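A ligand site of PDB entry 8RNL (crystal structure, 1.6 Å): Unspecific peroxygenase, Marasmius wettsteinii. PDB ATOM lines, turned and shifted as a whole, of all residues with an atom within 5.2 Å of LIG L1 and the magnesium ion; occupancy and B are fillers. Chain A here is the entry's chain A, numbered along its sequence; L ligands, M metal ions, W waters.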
ATOM      1  N   PRO A  20     -19.266  12.740 -19.580  1.00  0.00           N
ATOM      2  CA  PRO A  20     -18.456  13.915 -19.328  1.00  0.00           C
ATOM      3  C   PRO A  20     -16.954  13.716 -19.566  1.00  0.00           C
ATOM      4  O   PRO A  20     -16.181  14.641 -19.367  1.00  0.00           O
ATOM      5  CB  PRO A  20     -18.748  14.155 -17.843  1.00  0.00           C
ATOM      6  CG  PRO A  20     -18.826  12.747 -17.277  1.00  0.00           C
ATOM      7  CD  PRO A  20     -19.549  11.959 -18.360  1.00  0.00           C
ATOM      8  N   CYS A  21     -16.575  12.499 -19.995  1.00  0.00           N
ATOM      9  CA  CYS A  21     -15.178  12.135 -20.162  1.00  0.00           C
ATOM     10  C   CYS A  21     -14.778  12.123 -21.625  1.00  0.00           C
ATOM     11  O   CYS A  21     -15.257  11.278 -22.378  1.00  0.00           O
ATOM     12  CB  CYS A  21     -14.891  10.767 -19.560  1.00  0.00           C
ATOM     13  SG  CYS A  21     -13.200  10.199 -19.879  1.00  0.00           S
ATOM     14  N   PRO A  22     -13.885  13.029 -22.083  1.00  0.00           N
ATOM     15  CA  PRO A  22     -13.433  13.011 -23.477  1.00  0.00           C
ATOM     16  C   PRO A  22     -12.653  11.747 -23.817  1.00  0.00           C
ATOM     17  O   PRO A  22     -12.624  11.295 -24.973  1.00  0.00           O
ATOM     18  CB  PRO A  22     -12.559  14.259 -23.607  1.00  0.00           C
ATOM     19  CG  PRO A  22     -12.067  14.504 -22.188  1.00  0.00           C
ATOM     20  CD  PRO A  22     -13.244  14.104 -21.319  1.00  0.00           C
ATOM     21  N   GLY A  23     -11.988  11.153 -22.839  1.00  0.00           N
ATOM     22  CA  GLY A  23     -11.218   9.940 -23.093  1.00  0.00           C
ATOM     23  C   GLY A  23     -12.101   8.791 -23.535  1.00  0.00           C
ATOM     24  O   GLY A  23     -11.840   8.152 -24.566  1.00  0.00           O
ATOM     25  N   LEU A  24     -13.148   8.503 -22.767  1.00  0.00           N
ATOM     26  CA  LEU A  24     -14.047   7.405 -23.078  1.00  0.00           C
ATOM     27  C   LEU A  24     -14.912   7.752 -24.281  1.00  0.00           C
ATOM     28  O   LEU A  24     -15.167   6.888 -25.117  1.00  0.00           O
ATOM     29  CB  LEU A  24     -14.888   7.047 -21.857  1.00  0.00           C
ATOM     30  CG  LEU A  24     -14.094   6.564 -20.650  1.00  0.00           C
ATOM     31  CD1 LEU A  24     -15.052   6.228 -19.529  1.00  0.00           C
ATOM     32  CD2 LEU A  24     -13.196   5.375 -20.977  1.00  0.00           C
ATOM     33  N   LEU A  27     -12.918   7.119 -27.414  1.00  0.00           N
ATOM     34  CA  LEU A  27     -12.806   5.699 -27.704  1.00  0.00           C
ATOM     35  C   LEU A  27     -14.083   5.188 -28.346  1.00  0.00           C
ATOM     36  O   LEU A  27     -14.016   4.373 -29.283  1.00  0.00           O
ATOM     37  CB  LEU A  27     -12.465   4.931 -26.426  1.00  0.00           C
ATOM     38  CG  LEU A  27     -11.049   5.163 -25.896  1.00  0.00           C
ATOM     39  CD1 LEU A  27     -10.894   4.542 -24.526  1.00  0.00           C
ATOM     40  CD2 LEU A  27      -9.978   4.596 -26.849  1.00  0.00           C
ATOM     41  N   ILE A  45     -13.313  -1.343 -20.952  1.00  0.00           N
ATOM     42  CA  ILE A  45     -12.576  -0.099 -20.820  1.00  0.00           C
ATOM     43  C   ILE A  45     -11.062  -0.338 -20.810  1.00  0.00           C
ATOM     44  O   ILE A  45     -10.307   0.388 -21.454  1.00  0.00           O
ATOM     45  CB  ILE A  45     -13.035   0.660 -19.563  1.00  0.00           C
ATOM     46  CG1 ILE A  45     -14.481   1.136 -19.710  1.00  0.00           C
ATOM     47  CG2 ILE A  45     -12.088   1.794 -19.244  1.00  0.00           C
ATOM     48  CD1 ILE A  45     -15.103   1.593 -18.421  1.00  0.00           C
ATOM     49  N   TYR A  53      -4.869   4.146 -26.603  1.00  0.00           N
ATOM     50  CA  TYR A  53      -4.045   5.169 -25.997  1.00  0.00           C
ATOM     51  C   TYR A  53      -2.773   4.614 -25.347  1.00  0.00           C
ATOM     52  O   TYR A  53      -1.914   5.399 -24.928  1.00  0.00           O
ATOM     53  CB  TYR A  53      -4.830   5.868 -24.876  1.00  0.00           C
ATOM     54  CG  TYR A  53      -6.117   6.561 -25.248  1.00  0.00           C
ATOM     55  CD1 TYR A  53      -6.249   7.328 -26.398  1.00  0.00           C
ATOM     56  CD2 TYR A  53      -7.203   6.527 -24.388  1.00  0.00           C
ATOM     57  CE1 TYR A  53      -7.414   8.014 -26.687  1.00  0.00           C
ATOM     58  CE2 TYR A  53      -8.367   7.234 -24.653  1.00  0.00           C
ATOM     59  CZ  TYR A  53      -8.483   7.971 -25.811  1.00  0.00           C
ATOM     60  OH  TYR A  53      -9.644   8.637 -26.090  1.00  0.00           O
ATOM     61  N   VAL A  55      -2.880   3.221 -22.496  1.00  0.00           N
ATOM     62  CA  VAL A  55      -3.100   3.385 -21.063  1.00  0.00           C
ATOM     63  C   VAL A  55      -3.283   1.992 -20.452  1.00  0.00           C
ATOM     64  O   VAL A  55      -4.034   1.168 -20.970  1.00  0.00           O
ATOM     65  CB  VAL A  55      -4.285   4.321 -20.773  1.00  0.00           C
ATOM     66  CG1 VAL A  55      -4.634   4.335 -19.298  1.00  0.00           C
ATOM     67  CG2 VAL A  55      -4.012   5.720 -21.263  1.00  0.00           C
ATOM     68  N   ILE A  59      -4.540   2.017 -13.853  1.00  0.00           N
ATOM     69  CA  ILE A  59      -5.369   3.205 -13.666  1.00  0.00           C
ATOM     70  C   ILE A  59      -6.795   2.908 -14.146  1.00  0.00           C
ATOM     71  O   ILE A  59      -7.747   3.388 -13.546  1.00  0.00           O
ATOM     72  CB  ILE A  59      -4.766   4.466 -14.315  1.00  0.00           C
ATOM     73  CG1 ILE A  59      -5.601   5.710 -13.978  1.00  0.00           C
ATOM     74  CG2 ILE A  59      -4.610   4.302 -15.816  1.00  0.00           C
ATOM     75  CD1 ILE A  59      -4.938   7.035 -14.269  1.00  0.00           C
ATOM     76  N   LEU A  60      -6.956   2.111 -15.207  1.00  0.00           N
ATOM     77  CA  LEU A  60      -8.271   1.897 -15.764  1.00  0.00           C
ATOM     78  C   LEU A  60      -9.136   0.984 -14.897  1.00  0.00           C
ATOM     79  O   LEU A  60     -10.354   1.140 -14.861  1.00  0.00           O
ATOM     80  CB  LEU A  60      -8.157   1.389 -17.200  1.00  0.00           C
ATOM     81  CG  LEU A  60      -7.512   2.372 -18.172  1.00  0.00           C
ATOM     82  CD1 LEU A  60      -7.383   1.772 -19.554  1.00  0.00           C
ATOM     83  CD2 LEU A  60      -8.287   3.697 -18.254  1.00  0.00           C
ATOM     84  N   ALA A  63     -10.082   3.457 -11.771  1.00  0.00           N
ATOM     85  CA  ALA A  63     -11.078   4.433 -12.163  1.00  0.00           C
ATOM     86  C   ALA A  63     -12.359   3.755 -12.653  1.00  0.00           C
ATOM     87  O   ALA A  63     -13.463   4.173 -12.337  1.00  0.00           O
ATOM     88  CB  ALA A  63     -10.509   5.342 -13.224  1.00  0.00           C
ATOM     89  N   GLY A  64     -12.198   2.697 -13.444  1.00  0.00           N
ATOM     90  CA  GLY A  64     -13.313   1.970 -14.017  1.00  0.00           C
ATOM     91  C   GLY A  64     -14.299   1.465 -12.964  1.00  0.00           C
ATOM     92  O   GLY A  64     -15.510   1.585 -13.131  1.00  0.00           O
ATOM     93  N   GLY A  67     -16.234   4.171 -11.552  1.00  0.00           N
ATOM     94  CA  GLY A  67     -17.243   4.553 -12.533  1.00  0.00           C
ATOM     95  C   GLY A  67     -18.439   3.616 -12.586  1.00  0.00           C
ATOM     96  O   GLY A  67     -19.554   4.037 -12.831  1.00  0.00           O
ATOM     97  N   LEU A  82     -21.839   8.292 -16.163  1.00  0.00           N
ATOM     98  CA  LEU A  82     -20.680   8.852 -15.481  1.00  0.00           C
ATOM     99  C   LEU A  82     -20.862  10.328 -15.109  1.00  0.00           C
ATOM    100  O   LEU A  82     -20.042  10.879 -14.377  1.00  0.00           O
ATOM    101  CB  LEU A  82     -19.467   8.684 -16.389  1.00  0.00           C
ATOM    102  CG  LEU A  82     -18.990   7.254 -16.576  1.00  0.00           C
ATOM    103  CD1 LEU A  82     -17.917   7.202 -17.640  1.00  0.00           C
ATOM    104  CD2 LEU A  82     -18.469   6.662 -15.274  1.00  0.00           C
ATOM    105  N   ILE A  88     -17.312  10.379  -9.617  1.00  0.00           N
ATOM    106  CA  ILE A  88     -16.111  10.959 -10.215  1.00  0.00           C
ATOM    107  C   ILE A  88     -16.393  12.394 -10.661  1.00  0.00           C
ATOM    108  O   ILE A  88     -15.575  13.279 -10.398  1.00  0.00           O
ATOM    109  CB  ILE A  88     -15.604  10.093 -11.379  1.00  0.00           C
ATOM    110  CG1 ILE A  88     -15.238   8.684 -10.898  1.00  0.00           C
ATOM    111  CG2 ILE A  88     -14.417  10.736 -12.072  1.00  0.00           C
ATOM    112  CD1 ILE A  88     -14.972   7.711 -12.043  1.00  0.00           C
ATOM    113  N   GLU A  89     -17.527  12.624 -11.325  1.00  0.00           N
ATOM    114  CA  GLU A  89     -17.832  13.937 -11.881  1.00  0.00           C
ATOM    115  C   GLU A  89     -17.787  14.993 -10.764  1.00  0.00           C
ATOM    116  O   GLU A  89     -18.263  14.781  -9.652  1.00  0.00           O
ATOM    117  CB  GLU A  89     -19.188  13.927 -12.587  1.00  0.00           C
ATOM    118  CG  GLU A  89     -19.411  15.142 -13.469  1.00  0.00           C
ATOM    119  CD  GLU A  89     -19.769  16.408 -12.711  1.00  0.00           C
ATOM    120  OE1 GLU A  89     -20.609  16.323 -11.765  1.00  0.00           O
ATOM    121  OE2 GLU A  89     -19.256  17.467 -13.084  1.00  0.00           O
ATOM    122  N   HIS A  90     -17.171  16.119 -11.099  1.00  0.00           N
ATOM    123  CA  HIS A  90     -16.818  17.166 -10.145  1.00  0.00           C
ATOM    124  C   HIS A  90     -16.977  18.544 -10.770  1.00  0.00           C
ATOM    125  O   HIS A  90     -16.966  18.732 -11.995  1.00  0.00           O
ATOM    126  CB  HIS A  90     -15.374  16.966  -9.682  1.00  0.00           C
ATOM    127  CG  HIS A  90     -14.404  16.879 -10.810  1.00  0.00           C
ATOM    128  ND1 HIS A  90     -14.023  17.972 -11.543  1.00  0.00           N
ATOM    129  CD2 HIS A  90     -13.797  15.812 -11.398  1.00  0.00           C
ATOM    130  CE1 HIS A  90     -13.227  17.593 -12.522  1.00  0.00           C
ATOM    131  NE2 HIS A  90     -13.059  16.276 -12.440  1.00  0.00           N
ATOM    132  N   ASP A  91     -17.018  19.545  -9.883  1.00  0.00           N
ATOM    133  CA  ASP A  91     -16.985  20.934 -10.288  1.00  0.00           C
ATOM    134  C   ASP A  91     -15.585  21.306 -10.775  1.00  0.00           C
ATOM    135  O   ASP A  91     -14.625  20.564 -10.588  1.00  0.00           O
ATOM    136  CB  ASP A  91     -17.367  21.823  -9.098  1.00  0.00           C
ATOM    137  CG  ASP A  91     -18.769  21.555  -8.580  1.00  0.00           C
ATOM    138  OD1 ASP A  91     -19.626  21.177  -9.379  1.00  0.00           O
ATOM    139  OD2 ASP A  91     -18.991  21.773  -7.358  1.00  0.00           O
ATOM    140  N   SER A  93     -14.512  21.507 -13.840  1.00  0.00           N
ATOM    141  CA  SER A  93     -14.062  20.758 -15.003  1.00  0.00           C
ATOM    142  C   SER A  93     -13.410  21.697 -16.020  1.00  0.00           C
ATOM    143  O   SER A  93     -13.610  22.898 -15.975  1.00  0.00           O
ATOM    144  CB  SER A  93     -15.229  20.037 -15.646  1.00  0.00           C
ATOM    145  OG  SER A  93     -15.716  19.000 -14.799  1.00  0.00           O
ATOM    146  N   LEU A  94     -12.652  21.122 -16.956  1.00  0.00           N
ATOM    147  CA  LEU A  94     -11.918  21.874 -17.964  1.00  0.00           C
ATOM    148  C   LEU A  94     -12.811  22.298 -19.136  1.00  0.00           C
ATOM    149  O   LEU A  94     -12.458  23.235 -19.832  1.00  0.00           O
ATOM    150  CB  LEU A  94     -10.793  20.988 -18.508  1.00  0.00           C
ATOM    151  CG  LEU A  94      -9.767  20.526 -17.469  1.00  0.00           C
ATOM    152  CD1 LEU A  94      -8.940  19.364 -18.007  1.00  0.00           C
ATOM    153  CD2 LEU A  94      -8.867  21.654 -17.039  1.00  0.00           C
ATOM    154  N   SER A  95     -13.908  21.570 -19.368  1.00  0.00           N
ATOM    155  CA  SER A  95     -14.688  21.727 -20.592  1.00  0.00           C
ATOM    156  C   SER A  95     -16.196  21.562 -20.365  1.00  0.00           C
ATOM    157  O   SER A  95     -16.949  21.610 -21.331  1.00  0.00           O
ATOM    158  CB  SER A  95     -14.182  20.768 -21.659  1.00  0.00           C
ATOM    159  OG  SER A  95     -14.532  19.410 -21.377  1.00  0.00           O
ATOM    160  N   ARG A  96     -16.617  21.348 -19.119  1.00  0.00           N
ATOM    161  CA  ARG A  96     -18.018  21.202 -18.733  1.00  0.00           C
ATOM    162  C   ARG A  96     -18.333  22.239 -17.651  1.00  0.00           C
ATOM    163  O   ARG A  96     -17.428  22.716 -16.983  1.00  0.00           O
ATOM    164  CB  ARG A  96     -18.318  19.809 -18.170  1.00  0.00           C
ATOM    165  CG  ARG A  96     -18.679  18.735 -19.189  1.00  0.00           C
ATOM    166  CD  ARG A  96     -17.638  18.488 -20.254  1.00  0.00           C
ATOM    167  NE  ARG A  96     -18.015  17.328 -21.048  1.00  0.00           N
ATOM    168  CZ  ARG A  96     -17.357  16.881 -22.111  1.00  0.00           C
ATOM    169  NH1 ARG A  96     -16.235  17.444 -22.517  1.00  0.00           N
ATOM    170  NH2 ARG A  96     -17.875  15.861 -22.775  1.00  0.00           N
ATOM    171  N   GLU A  97     -19.631  22.529 -17.491  1.00  0.00           N
ATOM    172  CA  GLU A  97     -20.092  23.439 -16.455  1.00  0.00           C
ATOM    173  C   GLU A  97     -20.345  22.643 -15.173  1.00  0.00           C
ATOM    174  O   GLU A  97     -20.558  21.445 -15.210  1.00  0.00           O
ATOM    175  CB  GLU A  97     -21.370  24.176 -16.902  1.00  0.00           C
ATOM    176  CG  GLU A  97     -21.194  24.938 -18.205  1.00  0.00           C
ATOM    177  CD  GLU A  97     -22.473  25.583 -18.731  1.00  0.00           C
ATOM    178  OE1 GLU A  97     -23.560  24.957 -18.625  1.00  0.00           O
ATOM    179  OE2 GLU A  97     -22.377  26.698 -19.285  1.00  0.00           O
ATOM    180  N   ASN A 104     -23.324  19.594 -16.796  1.00  0.00           N
ATOM    181  CA  ASN A 104     -22.097  18.946 -16.358  1.00  0.00           C
ATOM    182  C   ASN A 104     -21.699  17.810 -17.283  1.00  0.00           C
ATOM    183  O   ASN A 104     -20.789  17.065 -16.954  1.00  0.00           O
ATOM    184  CB  ASN A 104     -22.192  18.448 -14.919  1.00  0.00           C
ATOM    185  CG  ASN A 104     -23.047  17.208 -14.760  1.00  0.00           C
ATOM    186  OD1 ASN A 104     -23.870  16.907 -15.615  1.00  0.00           O
ATOM    187  ND2 ASN A 104     -22.851  16.455 -13.691  1.00  0.00           N
ATOM    188  N   GLU A 161      -6.899  14.038 -14.496  1.00  0.00           N
ATOM    189  CA  GLU A 161      -7.496  14.321 -15.804  1.00  0.00           C
ATOM    190  C   GLU A 161      -6.571  15.193 -16.652  1.00  0.00           C
ATOM    191  O   GLU A 161      -6.415  14.966 -17.861  1.00  0.00           O
ATOM    192  CB  GLU A 161      -8.896  14.889 -15.586  1.00  0.00           C
ATOM    193  CG  GLU A 161      -9.819  13.810 -15.029  1.00  0.00           C
ATOM    194  CD  GLU A 161     -11.091  14.212 -14.316  1.00  0.00           C
ATOM    195  OE1 GLU A 161     -11.304  15.398 -14.110  1.00  0.00           O
ATOM    196  OE2 GLU A 161     -11.846  13.278 -13.940  1.00  0.00           O
ATOM    197  N   SER A 162      -5.942  16.208 -16.058  1.00  0.00           N
ATOM    198  CA  SER A 162      -4.983  17.024 -16.781  1.00  0.00           C
ATOM    199  C   SER A 162      -3.790  16.174 -17.229  1.00  0.00           C
ATOM    200  O   SER A 162      -3.341  16.293 -18.366  1.00  0.00           O
ATOM    201  CB  SER A 162      -4.546  18.227 -15.982  1.00  0.00           C
ATOM    202  OG  SER A 162      -5.653  19.100 -15.761  1.00  0.00           O
ATOM    203  N   PHE A 164      -3.863  13.095 -17.919  1.00  0.00           N
ATOM    204  CA  PHE A 164      -4.336  12.265 -19.019  1.00  0.00           C
ATOM    205  C   PHE A 164      -4.195  12.986 -20.359  1.00  0.00           C
ATOM    206  O   PHE A 164      -3.677  12.426 -21.331  1.00  0.00           O
ATOM    207  CB  PHE A 164      -5.787  11.832 -18.802  1.00  0.00           C
ATOM    208  CG  PHE A 164      -5.982  10.466 -18.214  1.00  0.00           C
ATOM    209  CD1 PHE A 164      -5.169   9.409 -18.625  1.00  0.00           C
ATOM    210  CD2 PHE A 164      -7.072  10.202 -17.393  1.00  0.00           C
ATOM    211  CE1 PHE A 164      -5.394   8.129 -18.143  1.00  0.00           C
ATOM    212  CE2 PHE A 164      -7.287   8.915 -16.919  1.00  0.00           C
ATOM    213  CZ  PHE A 164      -6.441   7.895 -17.279  1.00  0.00           C
ATOM    214  N   TYR A 165      -4.697  14.223 -20.470  1.00  0.00           N
ATOM    215  CA  TYR A 165      -4.621  14.851 -21.782  1.00  0.00           C
ATOM    216  C   TYR A 165      -3.179  15.186 -22.174  1.00  0.00           C
ATOM    217  O   TYR A 165      -2.845  15.080 -23.356  1.00  0.00           O
ATOM    218  CB  TYR A 165      -5.579  16.040 -21.951  1.00  0.00           C
ATOM    219  CG  TYR A 165      -5.195  17.337 -21.305  1.00  0.00           C
ATOM    220  CD1 TYR A 165      -4.167  18.142 -21.779  1.00  0.00           C
ATOM    221  CD2 TYR A 165      -5.905  17.797 -20.217  1.00  0.00           C
ATOM    222  CE1 TYR A 165      -3.846  19.354 -21.185  1.00  0.00           C
ATOM    223  CE2 TYR A 165      -5.608  18.999 -19.608  1.00  0.00           C
ATOM    224  CZ  TYR A 165      -4.575  19.785 -20.074  1.00  0.00           C
ATOM    225  OH  TYR A 165      -4.210  20.998 -19.501  1.00  0.00           O
ATOM    226  N   VAL A 168      -1.829  11.264 -23.079  1.00  0.00           N
ATOM    227  CA  VAL A 168      -2.440  10.454 -24.115  1.00  0.00           C
ATOM    228  C   VAL A 168      -2.344  11.145 -25.476  1.00  0.00           C
ATOM    229  O   VAL A 168      -2.248  10.461 -26.504  1.00  0.00           O
ATOM    230  CB  VAL A 168      -3.886  10.085 -23.750  1.00  0.00           C
ATOM    231  CG1 VAL A 168      -4.626   9.460 -24.907  1.00  0.00           C
ATOM    232  CG2 VAL A 168      -3.937   9.187 -22.525  1.00  0.00           C
ATOM    233  N   PHE A 187      -9.106  16.632 -29.442  1.00  0.00           N
ATOM    234  CA  PHE A 187      -9.535  15.666 -28.450  1.00  0.00           C
ATOM    235  C   PHE A 187     -10.755  16.184 -27.699  1.00  0.00           C
ATOM    236  O   PHE A 187     -11.759  15.476 -27.575  1.00  0.00           O
ATOM    237  CB  PHE A 187      -8.339  15.328 -27.560  1.00  0.00           C
ATOM    238  CG  PHE A 187      -8.604  14.401 -26.404  1.00  0.00           C
ATOM    239  CD1 PHE A 187      -8.877  13.061 -26.621  1.00  0.00           C
ATOM    240  CD2 PHE A 187      -8.569  14.857 -25.095  1.00  0.00           C
ATOM    241  CE1 PHE A 187      -9.128  12.191 -25.557  1.00  0.00           C
ATOM    242  CE2 PHE A 187      -8.789  13.982 -24.049  1.00  0.00           C
ATOM    243  CZ  PHE A 187      -9.078  12.655 -24.273  1.00  0.00           C
ATOM    244  N   PHE A 188     -10.690  17.412 -27.175  1.00  0.00           N
ATOM    245  CA  PHE A 188     -11.791  17.977 -26.398  1.00  0.00           C
ATOM    246  C   PHE A 188     -12.953  18.418 -27.289  1.00  0.00           C
ATOM    247  O   PHE A 188     -14.107  18.120 -26.992  1.00  0.00           O
ATOM    248  CB  PHE A 188     -11.306  19.177 -25.574  1.00  0.00           C
ATOM    249  CG  PHE A 188     -10.683  18.846 -24.232  1.00  0.00           C
ATOM    250  CD1 PHE A 188     -11.462  18.660 -23.119  1.00  0.00           C
ATOM    251  CD2 PHE A 188      -9.310  18.684 -24.108  1.00  0.00           C
ATOM    252  CE1 PHE A 188     -10.887  18.368 -21.895  1.00  0.00           C
ATOM    253  CE2 PHE A 188      -8.738  18.379 -22.889  1.00  0.00           C
ATOM    254  CZ  PHE A 188      -9.540  18.235 -21.773  1.00  0.00           C
HETATM  255  C1  LIG L   1     -13.112  13.475 -17.105  1.00  0.00           C
HETATM  256  C2  LIG L   1     -14.393   8.985 -15.967  1.00  0.00           C
HETATM  257  C3  LIG L   1     -10.631   7.307 -18.490  1.00  0.00           C
HETATM  258  C4  LIG L   1      -9.511  11.808 -19.802  1.00  0.00           C
HETATM  259  C5  LIG L   1     -13.795  12.401 -16.642  1.00  0.00           C
HETATM  260  C6  LIG L   1     -15.001  12.462 -15.894  1.00  0.00           C
HETATM  261  C7  LIG L   1     -15.392  11.226 -15.569  1.00  0.00           C
HETATM  262  C8  LIG L   1     -14.391  10.339 -16.116  1.00  0.00           C
HETATM  263  C9  LIG L   1     -16.630  10.871 -14.788  1.00  0.00           C
HETATM  264  C10 LIG L   1     -15.735  13.745 -15.561  1.00  0.00           C
HETATM  265  C11 LIG L   1     -15.010  14.521 -14.429  1.00  0.00           C
HETATM  266  C12 LIG L   1     -15.341  15.999 -14.501  1.00  0.00           C
HETATM  267  O1  LIG L   1     -16.291  16.466 -13.774  1.00  0.00           O
HETATM  268  O2  LIG L   1     -14.743  16.763 -15.310  1.00  0.00           O
HETATM  269  C13 LIG L   1     -13.433   8.140 -16.524  1.00  0.00           C
HETATM  270  C14 LIG L   1     -13.432   6.716 -16.278  1.00  0.00           C
HETATM  271  C15 LIG L   1     -12.394   6.226 -17.002  1.00  0.00           C
HETATM  272  C16 LIG L   1     -11.739   7.390 -17.660  1.00  0.00           C
HETATM  273  C17 LIG L   1     -14.416   5.928 -15.481  1.00  0.00           C
HETATM  274  C18 LIG L   1     -11.983   4.811 -16.967  1.00  0.00           C
HETATM  275  C19 LIG L   1     -10.726   4.583 -16.784  1.00  0.00           C
HETATM  276  C20 LIG L   1     -10.042   8.349 -19.160  1.00  0.00           C
HETATM  277  C21 LIG L   1      -9.032   8.258 -20.120  1.00  0.00           C
HETATM  278  C22 LIG L   1      -8.727   9.539 -20.501  1.00  0.00           C
HETATM  279  C23 LIG L   1      -9.533  10.451 -19.751  1.00  0.00           C
HETATM  280  C24 LIG L   1      -8.426   6.969 -20.674  1.00  0.00           C
HETATM  281  C25 LIG L   1      -7.681   9.819 -21.517  1.00  0.00           C
HETATM  282  C26 LIG L   1      -7.266  10.994 -21.891  1.00  0.00           C
HETATM  283  C27 LIG L   1     -10.394  12.662 -19.104  1.00  0.00           C
HETATM  284  C28 LIG L   1     -10.234  14.145 -19.141  1.00  0.00           C
HETATM  285  C29 LIG L   1     -11.284  14.595 -18.388  1.00  0.00           C
HETATM  286  C30 LIG L   1     -11.985  13.396 -17.913  1.00  0.00           C
HETATM  287  C31 LIG L   1      -9.197  14.940 -19.863  1.00  0.00           C
HETATM  288  C32 LIG L   1     -11.601  16.025 -17.999  1.00  0.00           C
HETATM  289  C33 LIG L   1     -12.768  16.645 -18.719  1.00  0.00           C
HETATM  290  C34 LIG L   1     -13.025  18.046 -18.205  1.00  0.00           C
HETATM  291  O3  LIG L   1     -12.478  18.400 -17.119  1.00  0.00           O
HETATM  292  O4  LIG L   1     -13.793  18.776 -18.864  1.00  0.00           O
HETATM  293  N1  LIG L   1     -13.433  11.071 -16.724  1.00  0.00           N
HETATM  294  N2  LIG L   1     -12.423   8.487 -17.308  1.00  0.00           N
HETATM  295  N3  LIG L   1     -10.326   9.666 -18.982  1.00  0.00           N
HETATM  296  N4  LIG L   1     -11.430  12.234 -18.339  1.00  0.00           N
HETATM  297 FE1  LIG L   1     -11.976  10.413 -17.953  1.00  0.00          FE
HETATM  298  O1  LG2 L   2     -10.671  10.522 -16.032  1.00  0.00           O
HETATM  299  O2  LG2 L   2     -11.405  10.867 -13.971  1.00  0.00           O
HETATM  300  C1  LG2 L   2     -10.558  10.415 -14.752  1.00  0.00           C
HETATM  301  C2  LG2 L   2      -9.323   9.765 -14.137  1.00  0.00           C
HETATM  302  C3  LG2 L   2      -9.321   9.671 -12.614  1.00  0.00           C
HETATM  303  C4  LG2 L   2     -10.064   8.450 -12.087  1.00  0.00           C
HETATM  304  C5  LG2 L   2     -10.658   8.579 -10.682  1.00  0.00           C
HETATM  305  C6  LG2 L   2     -10.302   7.448  -9.734  1.00  0.00           C
HETATM  306  C7  LG2 L   2      -9.571   7.849  -8.477  1.00  0.00           C
HETATM  307  C8  LG2 L   2      -8.297   8.657  -8.693  1.00  0.00           C
HETATM  308  C9  LG2 L   2      -7.149   7.885  -9.299  1.00  0.00           C
HETATM  309  C10 LG2 L   2      -5.840   8.637  -9.313  1.00  0.00           C
HETATM  310  C11 LG2 L   2      -5.129   8.704  -7.983  1.00  0.00           C
HETATM  311  C12 LG2 L   2      -3.642   8.935  -8.098  1.00  0.00           C
HETATM  312 MG    MG M   1     -17.518  18.175 -13.954  1.00  0.00          MG
HETATM  313  O   HOH W   1     -18.213  17.444 -15.808  1.00  0.00           O
HETATM  314  O   HOH W   2     -16.373  16.818 -17.720  1.00  0.00           O
HETATM  315  O   HOH W   3     -18.391  20.067 -14.163  1.00  0.00           O
HETATM  316  O   HOH W   4     -11.065  18.027 -14.924  1.00  0.00           O
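The side-chain carboxylate (OE1) of Glu 89 is in hydrogen-bond range of the side-chain amide nitrogen (ND2) of Asn 104 (3.0 Å). A ring nitrogen (NE2) of His 90 is in hydrogen-bond range of the side-chain carboxylate (OE1) of Glu 161, 2.6 Å away. The backbone NH of Gly 23 lies close to the side-chain sulfur of Cys 21, at 3.3 Å. SG of Cys 21 sits close to N of Leu 24, at 3.3 Å. OG of Ser 95 is in hydrogen-bond range of NH1 of Arg 96. The backbone carbonyl oxygen of Gly 23 lies within hydrogen-bond range of the side-chain hydroxyl of Tyr 53 (2.7 Å).
Water W4 lies within hydrogen-bond range of an oxygen (O3) of LIG L1 (2.6 Å) and the side-chain carboxylate (OE1) of Glu 161 (2.8 Å). Water W2 bridges the backbone carbonyl oxygen of Pro 20 and an oxygen (O2) of LIG L1.
FE1 of LIG L1 is bound by O1 of LG2 L2 (2.3 Å).
OE2 of Glu 89 is bound to the magnesium ion. Water W3 is bound to the magnesium ion. The magnesium ion is bound by water W1 (2.1 Å). The magnesium ion is bound by O1 of LIG L1 (2.1 Å). The magnesium ion is bound by O of His 90 (2.1 Å). The side-chain hydroxyl (OG) of Ser 93 is bound to the magnesium ion, 2.2 Å away. The magnesium ion has six donor atoms within binding distance.
An oxygen (O1) of LIG L1 lies close to the backbone NH of His 90 (2.8 Å). NE2 of His 90 sits close to O2 of LIG L1 (3.4 Å). The side-chain sulfur (SG) of Cys 21 is bound to an iron atom (FE1) of LIG L1, 2.3 Å away. An oxygen (O4) of LIG L1 sits at hydrogen-bond distance from the backbone NH of Ser 95. OG of Ser 95 sits at hydrogen-bond distance from O4 of LIG L1, 2.7 Å away. The backbone NH (N) of Leu 94 sits at hydrogen-bond distance from an oxygen (O3) of LIG L1 (2.7 Å). O2 of LG2 L2 sits close to OE2 of Glu 161 (2.5 Å).
Pro 20 touches LIG L1 (CG to C10, 3.7 Å). CD of Pro 22 touches C29 of LIG L1, 3.6 Å away. CA of Gly 23 touches C22 of LIG L1 (3.6 Å). Leu 24 touches LIG L1 (CD1 to C14, 3.7 Å). Ile 45 touches LIG L1. CD2 of Tyr 53 touches C24 of LIG L1, 3.9 Å away. Leu 60 touches LIG L1 (CD2 to C19, 3.0 Å). Ala 63 touches LIG L1. Leu 82 touches LIG L1 (O to C9, 3.4 Å). Ile 88 touches LIG L1. Arg 96 touches LIG L1. Glu 161 touches LIG L1 (OE2 to C1, 3.4 Å). Phe 164 touches LIG L1 (CD2 to C23, 3.4 Å). Val 168 touches LIG L1 (CG2 to C26, 3.8 Å). CZ of Phe 187 touches C26 of LIG L1, at 3.4 Å. Phe 188 touches LIG L1. Hydrophobic or aromatic side chains that line LIG L1: Pro 20, Pro 22, Leu 24, Ile 45, Tyr 53, Leu 60, Ala 63, Leu 82, Ile 88, His 90, Leu 94, Phe 164, Val 168, Phe 187 and Phe 188. 22 residues have an atom within 4 Å of LIG L1: Pro 20, Cys 21, Pro 22, Gly 23, Leu 24, Ile 45, Tyr 53, Leu 60, Ala 63, Leu 82, Ile 88, Glu 89, His 90, Ser 93, Leu 94, Ser 95, Arg 96, Glu 161, Phe 164, Val 168, Phe 187 and Phe 188. Along chain A the residues within 4 Å of LIG L1 span positions 20 to 188.
Within 4 Å of the magnesium ion: Glu 89, His 90 and Ser 93.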
